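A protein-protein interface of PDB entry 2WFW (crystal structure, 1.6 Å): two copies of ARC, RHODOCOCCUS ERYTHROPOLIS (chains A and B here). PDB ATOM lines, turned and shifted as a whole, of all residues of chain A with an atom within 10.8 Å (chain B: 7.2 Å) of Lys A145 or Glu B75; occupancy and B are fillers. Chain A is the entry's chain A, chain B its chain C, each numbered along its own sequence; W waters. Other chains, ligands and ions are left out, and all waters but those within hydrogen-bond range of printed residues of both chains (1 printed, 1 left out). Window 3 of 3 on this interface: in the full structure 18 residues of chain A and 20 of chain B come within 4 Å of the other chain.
Water W1 bridges the backbone carbonyl oxygen (O) of Ile A70 and the backbone NH (N) of Glu B92.
The backbone NH of Ile A70 lies within hydrogen-bond range of the backbone carbonyl oxygen of Glu B92 (3.0 Å).
The guanidinium group (NH1) of Arg B82 lies within salt-bridge range of the side-chain carboxylate (OE1) of Glu A141 (2.9 Å).
The side-chain carboxylate (OE2) of Glu B75 sits close to the backbone carbonyl oxygen (O) of Pro A144, 2.6 Å away.
OE1 of Glu B75 sits close to O of Ala A146, 3.0 Å away.
The side-chain carboxylate of Glu A147 sits close to the side-chain carboxylate of Asp B78 (3.2 Å).
6 positions are printed for both chains.
Ser A71 touches none of the printed residues of chain B.
Printed residues of chain B within 4 Å of Glu A141: Arg B82.
Arg A142 touches none of the printed residues of chain B.
Lys A145 touches one residue of chain B.
Of chain A, only Ile A143 (3.9 Å), Pro A144 (2.6 Å), Lys A145 (3.5 Å) and Ala A146 (3.0 Å) come within 4 Å of Glu B75.
No residue of chain A comes within 4 Å of Val B76.
Of the printed residues of chain A, Arg B82 touches Glu A141.
Printed residues of chain A within 4 Å of Leu B84: Ile A70 (3.9 Å).
No residue of chain A comes within 4 Å of Pro B108.
The nearest printed residue of chain B that does not touch Pro A144 is Leu B84 (4.9 Å).
Among the printed residues, pairs that only touch across the chains: Ile A70 with Leu B84 (3.9 Å), Ile A70 with Ile B94 (3.7 Å), Ile A143 with Glu B75 (3.9 Å), Ile A143 with Leu B77 (3.98 Å), Pro A144 with Asp B78 (3.9 Å) and Lys A145 with Glu B75 (3.5 Å).
Printed residues of chain A that touch a printed residue of chain B: Ile A70, Glu A141, Ile A143, Pro A144, Lys A145, Ala A146 and Glu A147.
Hydrophobic or aromatic side chains of chain A that line the printed part of chain B: Ile A70, Ile A143 and Pro A144.
Among the printed residues, 11 pairs touch across the chains.
Among the printed residues, Asp or Glu carboxylates within 4 Å of a Lys or Arg side-chain nitrogen of the other chain: Glu A141 with Arg B82 (2.9 Å).
O of Ser A129 sits at hydrogen-bond distance from N of Ile A143, at 2.9 Å.
The backbone NH (N) of Leu A131 sits at hydrogen-bond distance from the backbone carbonyl oxygen (O) of Glu A141, 2.9 Å away.
N of Arg B74 sits at hydrogen-bond distance from O of Leu B84 (2.8 Å).
OE2 of Glu B92 lies within salt-bridge range of NE of Arg B74 (3.3 Å).
O of Glu B75 sits at hydrogen-bond distance from N of Leu B84, 2.8 Å away.
The backbone carbonyl oxygen (O) of Arg B82 is in hydrogen-bond range of the backbone NH (N) of Leu B77.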
ATOM      1  N   ILE A  70      10.812  32.554  11.310  1.00  0.00           N
ATOM      2  CA  ILE A  70      10.364  31.378  10.576  1.00  0.00           C
ATOM      3  C   ILE A  70      10.909  31.417   9.162  1.00  0.00           C
ATOM      4  O   ILE A  70      10.918  32.471   8.520  1.00  0.00           O
ATOM      5  CB  ILE A  70       8.812  31.330  10.533  1.00  0.00           C
ATOM      6  CG1 ILE A  70       8.265  30.999  11.929  1.00  0.00           C
ATOM      7  CG2 ILE A  70       8.328  30.375   9.461  1.00  0.00           C
ATOM      8  CD1 ILE A  70       8.541  29.585  12.337  1.00  0.00           C
ATOM      9  N   SER A  71      11.391  30.260   8.705  1.00  0.00           N
ATOM     10  CA  SER A  71      11.881  30.089   7.352  1.00  0.00           C
ATOM     11  C   SER A  71      11.281  28.828   6.753  1.00  0.00           C
ATOM     12  O   SER A  71      10.801  27.981   7.489  1.00  0.00           O
ATOM     13  CB  SER A  71      13.387  29.960   7.365  1.00  0.00           C
ATOM     14  OG  SER A  71      13.885  30.376   6.125  1.00  0.00           O
ATOM     15  N   THR A  72      11.310  28.717   5.429  1.00  0.00           N
ATOM     16  CA  THR A  72      10.698  27.572   4.739  1.00  0.00           C
ATOM     17  C   THR A  72      11.785  26.612   4.244  1.00  0.00           C
ATOM     18  O   THR A  72      12.768  27.046   3.622  1.00  0.00           O
ATOM     19  CB  THR A  72       9.868  28.053   3.544  1.00  0.00           C
ATOM     20  OG1 THR A  72       8.859  28.973   3.994  1.00  0.00           O
ATOM     21  CG2 THR A  72       9.208  26.872   2.809  1.00  0.00           C
ATOM     22  N   LEU A  73      11.599  25.317   4.508  1.00  0.00           N
ATOM     23  CA  LEU A  73      12.555  24.303   4.081  1.00  0.00           C
ATOM     24  C   LEU A  73      12.534  24.140   2.543  1.00  0.00           C
ATOM     25  O   LEU A  73      11.461  23.990   1.935  1.00  0.00           O
ATOM     26  CB  LEU A  73      12.263  22.953   4.770  1.00  0.00           C
ATOM     27  CG  LEU A  73      13.161  21.765   4.361  1.00  0.00           C
ATOM     28  CD1 LEU A  73      14.646  22.061   4.689  1.00  0.00           C
ATOM     29  CD2 LEU A  73      12.707  20.485   5.030  1.00  0.00           C
ATOM     30  N   VAL A  86      14.566  29.060   3.079  1.00  0.00           N
ATOM     31  CA  VAL A  86      14.316  30.360   2.460  1.00  0.00           C
ATOM     32  C   VAL A  86      13.402  31.209   3.333  1.00  0.00           C
ATOM     33  O   VAL A  86      12.328  30.747   3.754  1.00  0.00           O
ATOM     34  CB  VAL A  86      13.782  30.217   1.003  1.00  0.00           C
ATOM     35  CG1 VAL A  86      12.634  29.220   0.950  1.00  0.00           C
ATOM     36  CG2 VAL A  86      13.373  31.573   0.418  1.00  0.00           C
ATOM     37  N   ASP A 107       9.595  16.763   6.743  1.00  0.00           N
ATOM     38  CA  ASP A 107      10.694  17.228   5.898  1.00  0.00           C
ATOM     39  C   ASP A 107      10.646  16.390   4.641  1.00  0.00           C
ATOM     40  O   ASP A 107      11.359  15.396   4.572  1.00  0.00           O
ATOM     41  CB  ASP A 107      12.057  17.068   6.594  1.00  0.00           C
ATOM     42  CG  ASP A 107      12.262  18.016   7.765  1.00  0.00           C
ATOM     43  OD1 ASP A 107      11.292  18.626   8.278  1.00  0.00           O
ATOM     44  OD2 ASP A 107      13.434  18.132   8.187  1.00  0.00           O
ATOM     45  N   PRO A 108       9.840  16.778   3.624  1.00  0.00           N
ATOM     46  CA  PRO A 108       9.235  17.889   2.874  1.00  0.00           C
ATOM     47  C   PRO A 108       9.678  19.342   3.120  1.00  0.00           C
ATOM     48  O   PRO A 108       9.550  19.828   4.235  1.00  0.00           O
ATOM     49  CB  PRO A 108       7.733  17.673   3.131  1.00  0.00           C
ATOM     50  CG  PRO A 108       7.625  16.108   3.368  1.00  0.00           C
ATOM     51  CD  PRO A 108       9.055  15.571   3.306  1.00  0.00           C
ATOM     52  N   GLU A 109      10.145  20.063   2.094  1.00  0.00           N
ATOM     53  CA  GLU A 109      10.230  19.656   0.698  1.00  0.00           C
ATOM     54  C   GLU A 109      11.312  18.625   0.470  1.00  0.00           C
ATOM     55  O   GLU A 109      11.187  17.494   0.918  1.00  0.00           O
ATOM     56  CB  GLU A 109      10.514  20.866  -0.193  1.00  0.00           C
ATOM     57  N   GLY A 127       9.060  22.710   2.091  1.00  0.00           N
ATOM     58  CA  GLY A 127       7.779  23.489   2.241  1.00  0.00           C
ATOM     59  C   GLY A 127       7.374  23.590   3.699  1.00  0.00           C
ATOM     60  O   GLY A 127       6.527  24.429   4.054  1.00  0.00           O
ATOM     61  N   ASP A 128       7.965  22.726   4.534  1.00  0.00           N
ATOM     62  CA  ASP A 128       7.759  22.764   5.988  1.00  0.00           C
ATOM     63  C   ASP A 128       8.224  24.130   6.516  1.00  0.00           C
ATOM     64  O   ASP A 128       9.224  24.673   6.026  1.00  0.00           O
ATOM     65  CB  ASP A 128       8.546  21.635   6.684  1.00  0.00           C
ATOM     66  CG  ASP A 128       7.890  20.258   6.542  1.00  0.00           C
ATOM     67  OD1 ASP A 128       6.801  20.160   5.964  1.00  0.00           O
ATOM     68  OD2 ASP A 128       8.493  19.266   7.024  1.00  0.00           O
ATOM     69  N   SER A 129       7.489  24.687   7.483  1.00  0.00           N
ATOM     70  CA  SER A 129       7.905  25.920   8.158  1.00  0.00           C
ATOM     71  C   SER A 129       8.785  25.557   9.337  1.00  0.00           C
ATOM     72  O   SER A 129       8.417  24.724  10.164  1.00  0.00           O
ATOM     73  CB  SER A 129       6.693  26.741   8.645  1.00  0.00           C
ATOM     74  OG  SER A 129       5.934  27.165   7.538  1.00  0.00           O
ATOM     75  N   LEU A 130       9.959  26.186   9.410  1.00  0.00           N
ATOM     76  CA  LEU A 130      10.889  25.896  10.481  1.00  0.00           C
ATOM     77  C   LEU A 130      11.213  27.140  11.296  1.00  0.00           C
ATOM     78  O   LEU A 130      11.463  28.198  10.732  1.00  0.00           O
ATOM     79  CB  LEU A 130      12.204  25.332   9.923  1.00  0.00           C
ATOM     80  CG  LEU A 130      12.131  24.091   9.027  1.00  0.00           C
ATOM     81  CD1 LEU A 130      13.525  23.648   8.548  1.00  0.00           C
ATOM     82  CD2 LEU A 130      11.384  22.961   9.776  1.00  0.00           C
ATOM     83  N   LEU A 131      11.219  26.981  12.616  1.00  0.00           N
ATOM     84  CA  LEU A 131      11.759  27.966  13.535  1.00  0.00           C
ATOM     85  C   LEU A 131      13.288  27.931  13.392  1.00  0.00           C
ATOM     86  O   LEU A 131      13.910  26.865  13.526  1.00  0.00           O
ATOM     87  CB  LEU A 131      11.397  27.583  14.965  1.00  0.00           C
ATOM     88  CG  LEU A 131      11.955  28.537  16.046  1.00  0.00           C
ATOM     89  CD1 LEU A 131      11.506  30.001  15.844  1.00  0.00           C
ATOM     90  CD2 LEU A 131      11.548  28.041  17.411  1.00  0.00           C
ATOM     91  N   GLU A 141      12.791  23.545  15.034  1.00  0.00           N
ATOM     92  CA  GLU A 141      11.431  23.042  15.241  1.00  0.00           C
ATOM     93  C   GLU A 141      10.601  23.235  13.980  1.00  0.00           C
ATOM     94  O   GLU A 141      10.744  24.233  13.281  1.00  0.00           O
ATOM     95  CB  GLU A 141      10.792  23.815  16.417  1.00  0.00           C
ATOM     96  CG  GLU A 141       9.445  23.274  16.898  1.00  0.00           C
ATOM     97  CD  GLU A 141       8.812  24.065  18.057  1.00  0.00           C
ATOM     98  OE1 GLU A 141       9.486  24.904  18.693  1.00  0.00           O
ATOM     99  OE2 GLU A 141       7.625  23.796  18.336  1.00  0.00           O
ATOM    100  N   ARG A 142       9.722  22.283  13.695  1.00  0.00           N
ATOM    101  CA  ARG A 142       8.763  22.448  12.617  1.00  0.00           C
ATOM    102  C   ARG A 142       7.437  22.984  13.177  1.00  0.00           C
ATOM    103  O   ARG A 142       6.957  22.507  14.201  1.00  0.00           O
ATOM    104  CB  ARG A 142       8.573  21.120  11.896  1.00  0.00           C
ATOM    105  CG  ARG A 142       7.530  21.160  10.829  1.00  0.00           C
ATOM    106  CD  ARG A 142       7.541  19.844  10.076  1.00  0.00           C
ATOM    107  NE  ARG A 142       7.267  18.705  10.957  1.00  0.00           N
ATOM    108  CZ  ARG A 142       7.439  17.428  10.611  1.00  0.00           C
ATOM    109  NH1 ARG A 142       7.893  17.116   9.400  1.00  0.00           N
ATOM    110  NH2 ARG A 142       7.150  16.454  11.476  1.00  0.00           N
ATOM    111  N   ILE A 143       6.875  23.980  12.489  1.00  0.00           N
ATOM    112  CA  ILE A 143       5.697  24.724  12.910  1.00  0.00           C
ATOM    113  C   ILE A 143       4.595  24.348  11.931  1.00  0.00           C
ATOM    114  O   ILE A 143       4.750  24.566  10.725  1.00  0.00           O
ATOM    115  CB  ILE A 143       5.979  26.252  12.837  1.00  0.00           C
ATOM    116  CG1 ILE A 143       7.241  26.596  13.646  1.00  0.00           C
ATOM    117  CG2 ILE A 143       4.767  27.086  13.299  1.00  0.00           C
ATOM    118  CD1 ILE A 143       7.126  26.323  15.169  1.00  0.00           C
ATOM    119  N   PRO A 144       3.485  23.774  12.440  1.00  0.00           N
ATOM    120  CA  PRO A 144       2.353  23.497  11.560  1.00  0.00           C
ATOM    121  C   PRO A 144       1.903  24.769  10.851  1.00  0.00           C
ATOM    122  O   PRO A 144       2.069  25.863  11.376  1.00  0.00           O
ATOM    123  CB  PRO A 144       1.283  23.008  12.532  1.00  0.00           C
ATOM    124  CG  PRO A 144       2.072  22.366  13.628  1.00  0.00           C
ATOM    125  CD  PRO A 144       3.210  23.335  13.820  1.00  0.00           C
ATOM    126  N   LYS A 145       1.348  24.620   9.658  1.00  0.00           N
ATOM    127  CA  LYS A 145       0.934  25.774   8.861  1.00  0.00           C
ATOM    128  C   LYS A 145      -0.457  26.380   9.139  1.00  0.00           C
ATOM    129  O   LYS A 145      -0.567  27.606   9.058  1.00  0.00           O
ATOM    130  CB  LYS A 145       1.140  25.511   7.363  1.00  0.00           C
ATOM    131  CG  LYS A 145       2.612  25.435   6.965  1.00  0.00           C
ATOM    132  CD  LYS A 145       2.800  25.021   5.506  1.00  0.00           C
ATOM    133  CE  LYS A 145       2.338  26.117   4.533  1.00  0.00           C
ATOM    134  NZ  LYS A 145       3.016  27.429   4.780  1.00  0.00           N
ATOM    135  N   ALA A 146      -1.530  25.636   9.460  1.00  0.00           N
ATOM    136  CA  ALA A 146      -1.736  24.165   9.658  1.00  0.00           C
ATOM    137  C   ALA A 146      -1.971  23.742  11.124  1.00  0.00           C
ATOM    138  O   ALA A 146      -1.645  24.485  12.053  1.00  0.00           O
ATOM    139  CB  ALA A 146      -0.703  23.273   8.957  1.00  0.00           C
ATOM    140  N   GLU A 147      -2.559  22.555  11.300  1.00  0.00           N
ATOM    141  CA  GLU A 147      -3.010  22.034  12.608  1.00  0.00           C
ATOM    142  C   GLU A 147      -3.856  23.010  13.439  1.00  0.00           C
ATOM    143  O   GLU A 147      -3.324  23.863  14.159  1.00  0.00           O
ATOM    144  CB  GLU A 147      -1.842  21.468  13.435  1.00  0.00           C
ATOM    145  CG  GLU A 147      -1.354  20.098  12.960  1.00  0.00           C
ATOM    146  CD  GLU A 147      -0.232  19.524  13.816  1.00  0.00           C
ATOM    147  OE1 GLU A 147       0.723  18.953  13.232  1.00  0.00           O
ATOM    148  OE2 GLU A 147      -0.302  19.639  15.063  1.00  0.00           O
ATOM    149  N   THR B  72       0.437  40.837  12.634  1.00  0.00           N
ATOM    150  CA  THR B  72      -0.858  40.191  12.445  1.00  0.00           C
ATOM    151  C   THR B  72      -0.796  38.739  12.873  1.00  0.00           C
ATOM    152  O   THR B  72       0.118  38.001  12.457  1.00  0.00           O
ATOM    153  CB  THR B  72      -1.293  40.300  10.968  1.00  0.00           C
ATOM    154  OG1 THR B  72      -1.251  41.674  10.565  1.00  0.00           O
ATOM    155  CG2 THR B  72      -2.726  39.770  10.789  1.00  0.00           C
ATOM    156  N   LEU B  73      -1.753  38.330  13.709  1.00  0.00           N
ATOM    157  CA  LEU B  73      -1.827  36.937  14.149  1.00  0.00           C
ATOM    158  C   LEU B  73      -2.162  36.015  12.980  1.00  0.00           C
ATOM    159  O   LEU B  73      -3.116  36.261  12.231  1.00  0.00           O
ATOM    160  CB  LEU B  73      -2.841  36.747  15.292  1.00  0.00           C
ATOM    161  CG  LEU B  73      -3.047  35.355  15.896  1.00  0.00           C
ATOM    162  CD1 LEU B  73      -1.736  34.798  16.449  1.00  0.00           C
ATOM    163  CD2 LEU B  73      -4.141  35.365  16.991  1.00  0.00           C
ATOM    164  N   ARG B  74      -1.369  34.955  12.834  1.00  0.00           N
ATOM    165  CA  ARG B  74      -1.688  33.918  11.853  1.00  0.00           C
ATOM    166  C   ARG B  74      -2.309  32.695  12.509  1.00  0.00           C
ATOM    167  O   ARG B  74      -3.301  32.154  12.008  1.00  0.00           O
ATOM    168  CB  ARG B  74      -0.453  33.518  11.055  1.00  0.00           C
ATOM    169  CG  ARG B  74       0.171  34.676  10.302  1.00  0.00           C
ATOM    170  CD  ARG B  74       0.936  34.182   9.081  1.00  0.00           C
ATOM    171  NE  ARG B  74       0.075  33.462   8.141  1.00  0.00           N
ATOM    172  CZ  ARG B  74      -0.783  34.038   7.299  1.00  0.00           C
ATOM    173  NH1 ARG B  74      -0.914  35.360   7.268  1.00  0.00           N
ATOM    174  NH2 ARG B  74      -1.520  33.286   6.488  1.00  0.00           N
ATOM    175  N   GLU B  75      -1.714  32.246  13.614  1.00  0.00           N
ATOM    176  CA  GLU B  75      -2.232  31.110  14.381  1.00  0.00           C
ATOM    177  C   GLU B  75      -1.635  31.065  15.778  1.00  0.00           C
ATOM    178  O   GLU B  75      -0.465  31.445  15.988  1.00  0.00           O
ATOM    179  CB  GLU B  75      -1.956  29.771  13.662  1.00  0.00           C
ATOM    180  CG  GLU B  75      -0.481  29.502  13.395  1.00  0.00           C
ATOM    181  CD  GLU B  75      -0.192  28.104  12.856  1.00  0.00           C
ATOM    182  OE1 GLU B  75      -1.135  27.366  12.507  1.00  0.00           O
ATOM    183  OE2 GLU B  75       0.998  27.735  12.789  1.00  0.00           O
ATOM    184  N   VAL B  76      -2.451  30.613  16.727  1.00  0.00           N
ATOM    185  CA  VAL B  76      -1.986  30.269  18.066  1.00  0.00           C
ATOM    186  C   VAL B  76      -1.475  28.823  18.001  1.00  0.00           C
ATOM    187  O   VAL B  76      -2.197  27.925  17.560  1.00  0.00           O
ATOM    188  CB  VAL B  76      -3.110  30.420  19.130  1.00  0.00           C
ATOM    189  CG1 VAL B  76      -2.644  29.917  20.495  1.00  0.00           C
ATOM    190  CG2 VAL B  76      -3.560  31.893  19.224  1.00  0.00           C
ATOM    191  N   LEU B  77      -0.233  28.601  18.427  1.00  0.00           N
ATOM    192  CA  LEU B  77       0.349  27.268  18.346  1.00  0.00           C
ATOM    193  C   LEU B  77      -0.353  26.289  19.290  1.00  0.00           C
ATOM    194  O   LEU B  77      -1.020  26.678  20.265  1.00  0.00           O
ATOM    195  CB  LEU B  77       1.873  27.287  18.574  1.00  0.00           C
ATOM    196  CG  LEU B  77       2.743  28.206  17.700  1.00  0.00           C
ATOM    197  CD1 LEU B  77       4.212  27.796  17.808  1.00  0.00           C
ATOM    198  CD2 LEU B  77       2.330  28.205  16.234  1.00  0.00           C
ATOM    199  N   ASP B  78      -0.196  25.014  18.973  1.00  0.00           N
ATOM    200  CA  ASP B  78      -0.842  23.928  19.692  1.00  0.00           C
ATOM    201  C   ASP B  78      -0.596  23.942  21.211  1.00  0.00           C
ATOM    202  O   ASP B  78      -1.451  23.506  21.977  1.00  0.00           O
ATOM    203  CB  ASP B  78      -0.497  22.572  19.044  1.00  0.00           C
ATOM    204  CG  ASP B  78       0.445  22.709  17.830  1.00  0.00           C
ATOM    205  OD1 ASP B  78       0.834  23.854  17.475  1.00  0.00           O
ATOM    206  OD2 ASP B  78       0.792  21.664  17.226  1.00  0.00           O
ATOM    207  N   ARG B  82       2.427  30.160  22.595  1.00  0.00           N
ATOM    208  CA  ARG B  82       3.150  30.890  21.544  1.00  0.00           C
ATOM    209  C   ARG B  82       2.207  31.117  20.375  1.00  0.00           C
ATOM    210  O   ARG B  82       1.183  30.444  20.254  1.00  0.00           O
ATOM    211  CB  ARG B  82       4.361  30.063  21.049  1.00  0.00           C
ATOM    212  CG  ARG B  82       5.390  29.738  22.126  1.00  0.00           C
ATOM    213  CD  ARG B  82       6.552  28.893  21.570  1.00  0.00           C
ATOM    214  NE  ARG B  82       6.058  27.565  21.225  1.00  0.00           N
ATOM    215  CZ  ARG B  82       6.682  26.675  20.452  1.00  0.00           C
ATOM    216  NH1 ARG B  82       7.870  26.947  19.902  1.00  0.00           N
ATOM    217  NH2 ARG B  82       6.110  25.506  20.229  1.00  0.00           N
ATOM    218  N   ALA B  83       2.547  32.070  19.515  1.00  0.00           N
ATOM    219  CA  ALA B  83       1.767  32.347  18.312  1.00  0.00           C
ATOM    220  C   ALA B  83       2.676  32.662  17.130  1.00  0.00           C
ATOM    221  O   ALA B  83       3.766  33.236  17.309  1.00  0.00           O
ATOM    222  CB  ALA B  83       0.797  33.519  18.570  1.00  0.00           C
ATOM    223  N   LEU B  84       2.202  32.310  15.938  1.00  0.00           N
ATOM    224  CA  LEU B  84       2.818  32.698  14.673  1.00  0.00           C
ATOM    225  C   LEU B  84       2.217  34.042  14.243  1.00  0.00           C
ATOM    226  O   LEU B  84       0.994  34.165  14.071  1.00  0.00           O
ATOM    227  CB  LEU B  84       2.519  31.623  13.614  1.00  0.00           C
ATOM    228  CG  LEU B  84       2.996  31.825  12.174  1.00  0.00           C
ATOM    229  CD1 LEU B  84       4.502  31.917  12.110  1.00  0.00           C
ATOM    230  CD2 LEU B  84       2.511  30.701  11.271  1.00  0.00           C
ATOM    231  N   VAL B  85       3.074  35.037  14.063  1.00  0.00           N
ATOM    232  CA  VAL B  85       2.636  36.370  13.639  1.00  0.00           C
ATOM    233  C   VAL B  85       3.368  36.774  12.354  1.00  0.00           C
ATOM    234  O   VAL B  85       4.483  36.277  12.082  1.00  0.00           O
ATOM    235  CB  VAL B  85       2.856  37.428  14.759  1.00  0.00           C
ATOM    236  CG1 VAL B  85       2.079  37.074  16.026  1.00  0.00           C
ATOM    237  CG2 VAL B  85       4.358  37.583  15.108  1.00  0.00           C
ATOM    238  N   GLU B  92       7.580  36.292   8.952  1.00  0.00           N
ATOM    239  CA  GLU B  92       6.872  35.453   9.929  1.00  0.00           C
ATOM    240  C   GLU B  92       7.776  35.126  11.117  1.00  0.00           C
ATOM    241  O   GLU B  92       8.978  34.902  10.950  1.00  0.00           O
ATOM    242  CB  GLU B  92       6.353  34.165   9.293  1.00  0.00           C
ATOM    243  CG  GLU B  92       5.235  34.383   8.264  1.00  0.00           C
ATOM    244  CD  GLU B  92       4.444  33.114   7.953  1.00  0.00           C
ATOM    245  OE1 GLU B  92       4.949  31.997   8.193  1.00  0.00           O
ATOM    246  OE2 GLU B  92       3.310  33.231   7.445  1.00  0.00           O
ATOM    247  N   ARG B  93       7.194  35.127  12.318  1.00  0.00           N
ATOM    248  CA  ARG B  93       7.946  34.851  13.544  1.00  0.00           C
ATOM    249  C   ARG B  93       7.041  34.134  14.524  1.00  0.00           C
ATOM    250  O   ARG B  93       5.805  34.280  14.473  1.00  0.00           O
ATOM    251  CB  ARG B  93       8.454  36.144  14.211  1.00  0.00           C
ATOM    252  CG  ARG B  93       9.473  36.941  13.389  1.00  0.00           C
ATOM    253  CD  ARG B  93      10.031  38.110  14.193  1.00  0.00           C
ATOM    254  NE  ARG B  93      10.924  37.674  15.258  1.00  0.00           N
ATOM    255  CZ  ARG B  93      12.245  37.558  15.129  1.00  0.00           C
ATOM    256  NH1 ARG B  93      12.843  37.795  13.961  1.00  0.00           N
ATOM    257  NH2 ARG B  93      12.973  37.171  16.171  1.00  0.00           N
ATOM    258  N   ILE B  94       7.663  33.383  15.425  1.00  0.00           N
ATOM    259  CA  ILE B  94       6.994  32.814  16.594  1.00  0.00           C
ATOM    260  C   ILE B  94       7.268  33.734  17.780  1.00  0.00           C
ATOM    261  O   ILE B  94       8.429  34.110  17.990  1.00  0.00           O
ATOM    262  CB  ILE B  94       7.528  31.397  16.968  1.00  0.00           C
ATOM    263  CG1 ILE B  94       7.367  30.426  15.794  1.00  0.00           C
ATOM    264  CG2 ILE B  94       6.795  30.860  18.203  1.00  0.00           C
ATOM    265  CD1 ILE B  94       5.961  30.452  15.195  1.00  0.00           C
ATOM    266  N   LEU B  97       3.038  34.434  24.038  1.00  0.00           N
ATOM    267  CA  LEU B  97       1.883  35.254  24.449  1.00  0.00           C
ATOM    268  C   LEU B  97       2.046  35.790  25.874  1.00  0.00           C
ATOM    269  O   LEU B  97       2.250  35.017  26.831  1.00  0.00           O
ATOM    270  CB  LEU B  97       0.582  34.441  24.384  1.00  0.00           C
ATOM    271  CG  LEU B  97       0.172  33.869  23.026  1.00  0.00           C
ATOM    272  CD1 LEU B  97      -1.103  33.053  23.185  1.00  0.00           C
ATOM    273  CD2 LEU B  97      -0.017  34.995  22.006  1.00  0.00           C
ATOM    274  N   ASP B 107      -8.392  33.970  15.296  1.00  0.00           N
ATOM    275  CA  ASP B 107      -8.284  34.300  13.860  1.00  0.00           C
ATOM    276  C   ASP B 107      -7.470  33.268  13.044  1.00  0.00           C
ATOM    277  O   ASP B 107      -6.939  32.320  13.621  1.00  0.00           O
ATOM    278  CB  ASP B 107      -7.799  35.738  13.635  1.00  0.00           C
ATOM    279  CG  ASP B 107      -6.774  36.172  14.643  1.00  0.00           C
ATOM    280  OD1 ASP B 107      -5.700  36.628  14.216  1.00  0.00           O
ATOM    281  OD2 ASP B 107      -7.037  36.067  15.856  1.00  0.00           O
ATOM    282  N   PRO B 108      -7.349  33.480  11.709  1.00  0.00           N
ATOM    283  CA  PRO B 108      -7.078  32.518  10.641  1.00  0.00           C
ATOM    284  C   PRO B 108      -6.725  31.055  10.990  1.00  0.00           C
ATOM    285  O   PRO B 108      -5.716  30.807  11.657  1.00  0.00           O
ATOM    286  CB  PRO B 108      -5.968  33.220   9.851  1.00  0.00           C
ATOM    287  CG  PRO B 108      -6.360  34.701   9.957  1.00  0.00           C
ATOM    288  CD  PRO B 108      -7.375  34.827  11.110  1.00  0.00           C
ATOM    289  N   GLU B 109      -7.539  30.090  10.544  1.00  0.00           N
ATOM    290  CA  GLU B 109      -8.811  30.294   9.811  1.00  0.00           C
ATOM    291  C   GLU B 109      -8.826  31.423   8.768  1.00  0.00           C
ATOM    292  O   GLU B 109      -8.100  31.389   7.771  1.00  0.00           O
ATOM    293  CB  GLU B 109      -9.981  30.463  10.798  1.00  0.00           C
ATOM    294  N   GLY B 127      -5.733  37.255  11.746  1.00  0.00           N
ATOM    295  CA  GLY B 127      -6.204  38.566  11.361  1.00  0.00           C
ATOM    296  C   GLY B 127      -6.136  39.615  12.453  1.00  0.00           C
ATOM    297  O   GLY B 127      -6.075  40.804  12.146  1.00  0.00           O
HETATM  298  O   HOH W   1       9.405  34.572   7.432  1.00  0.00           O
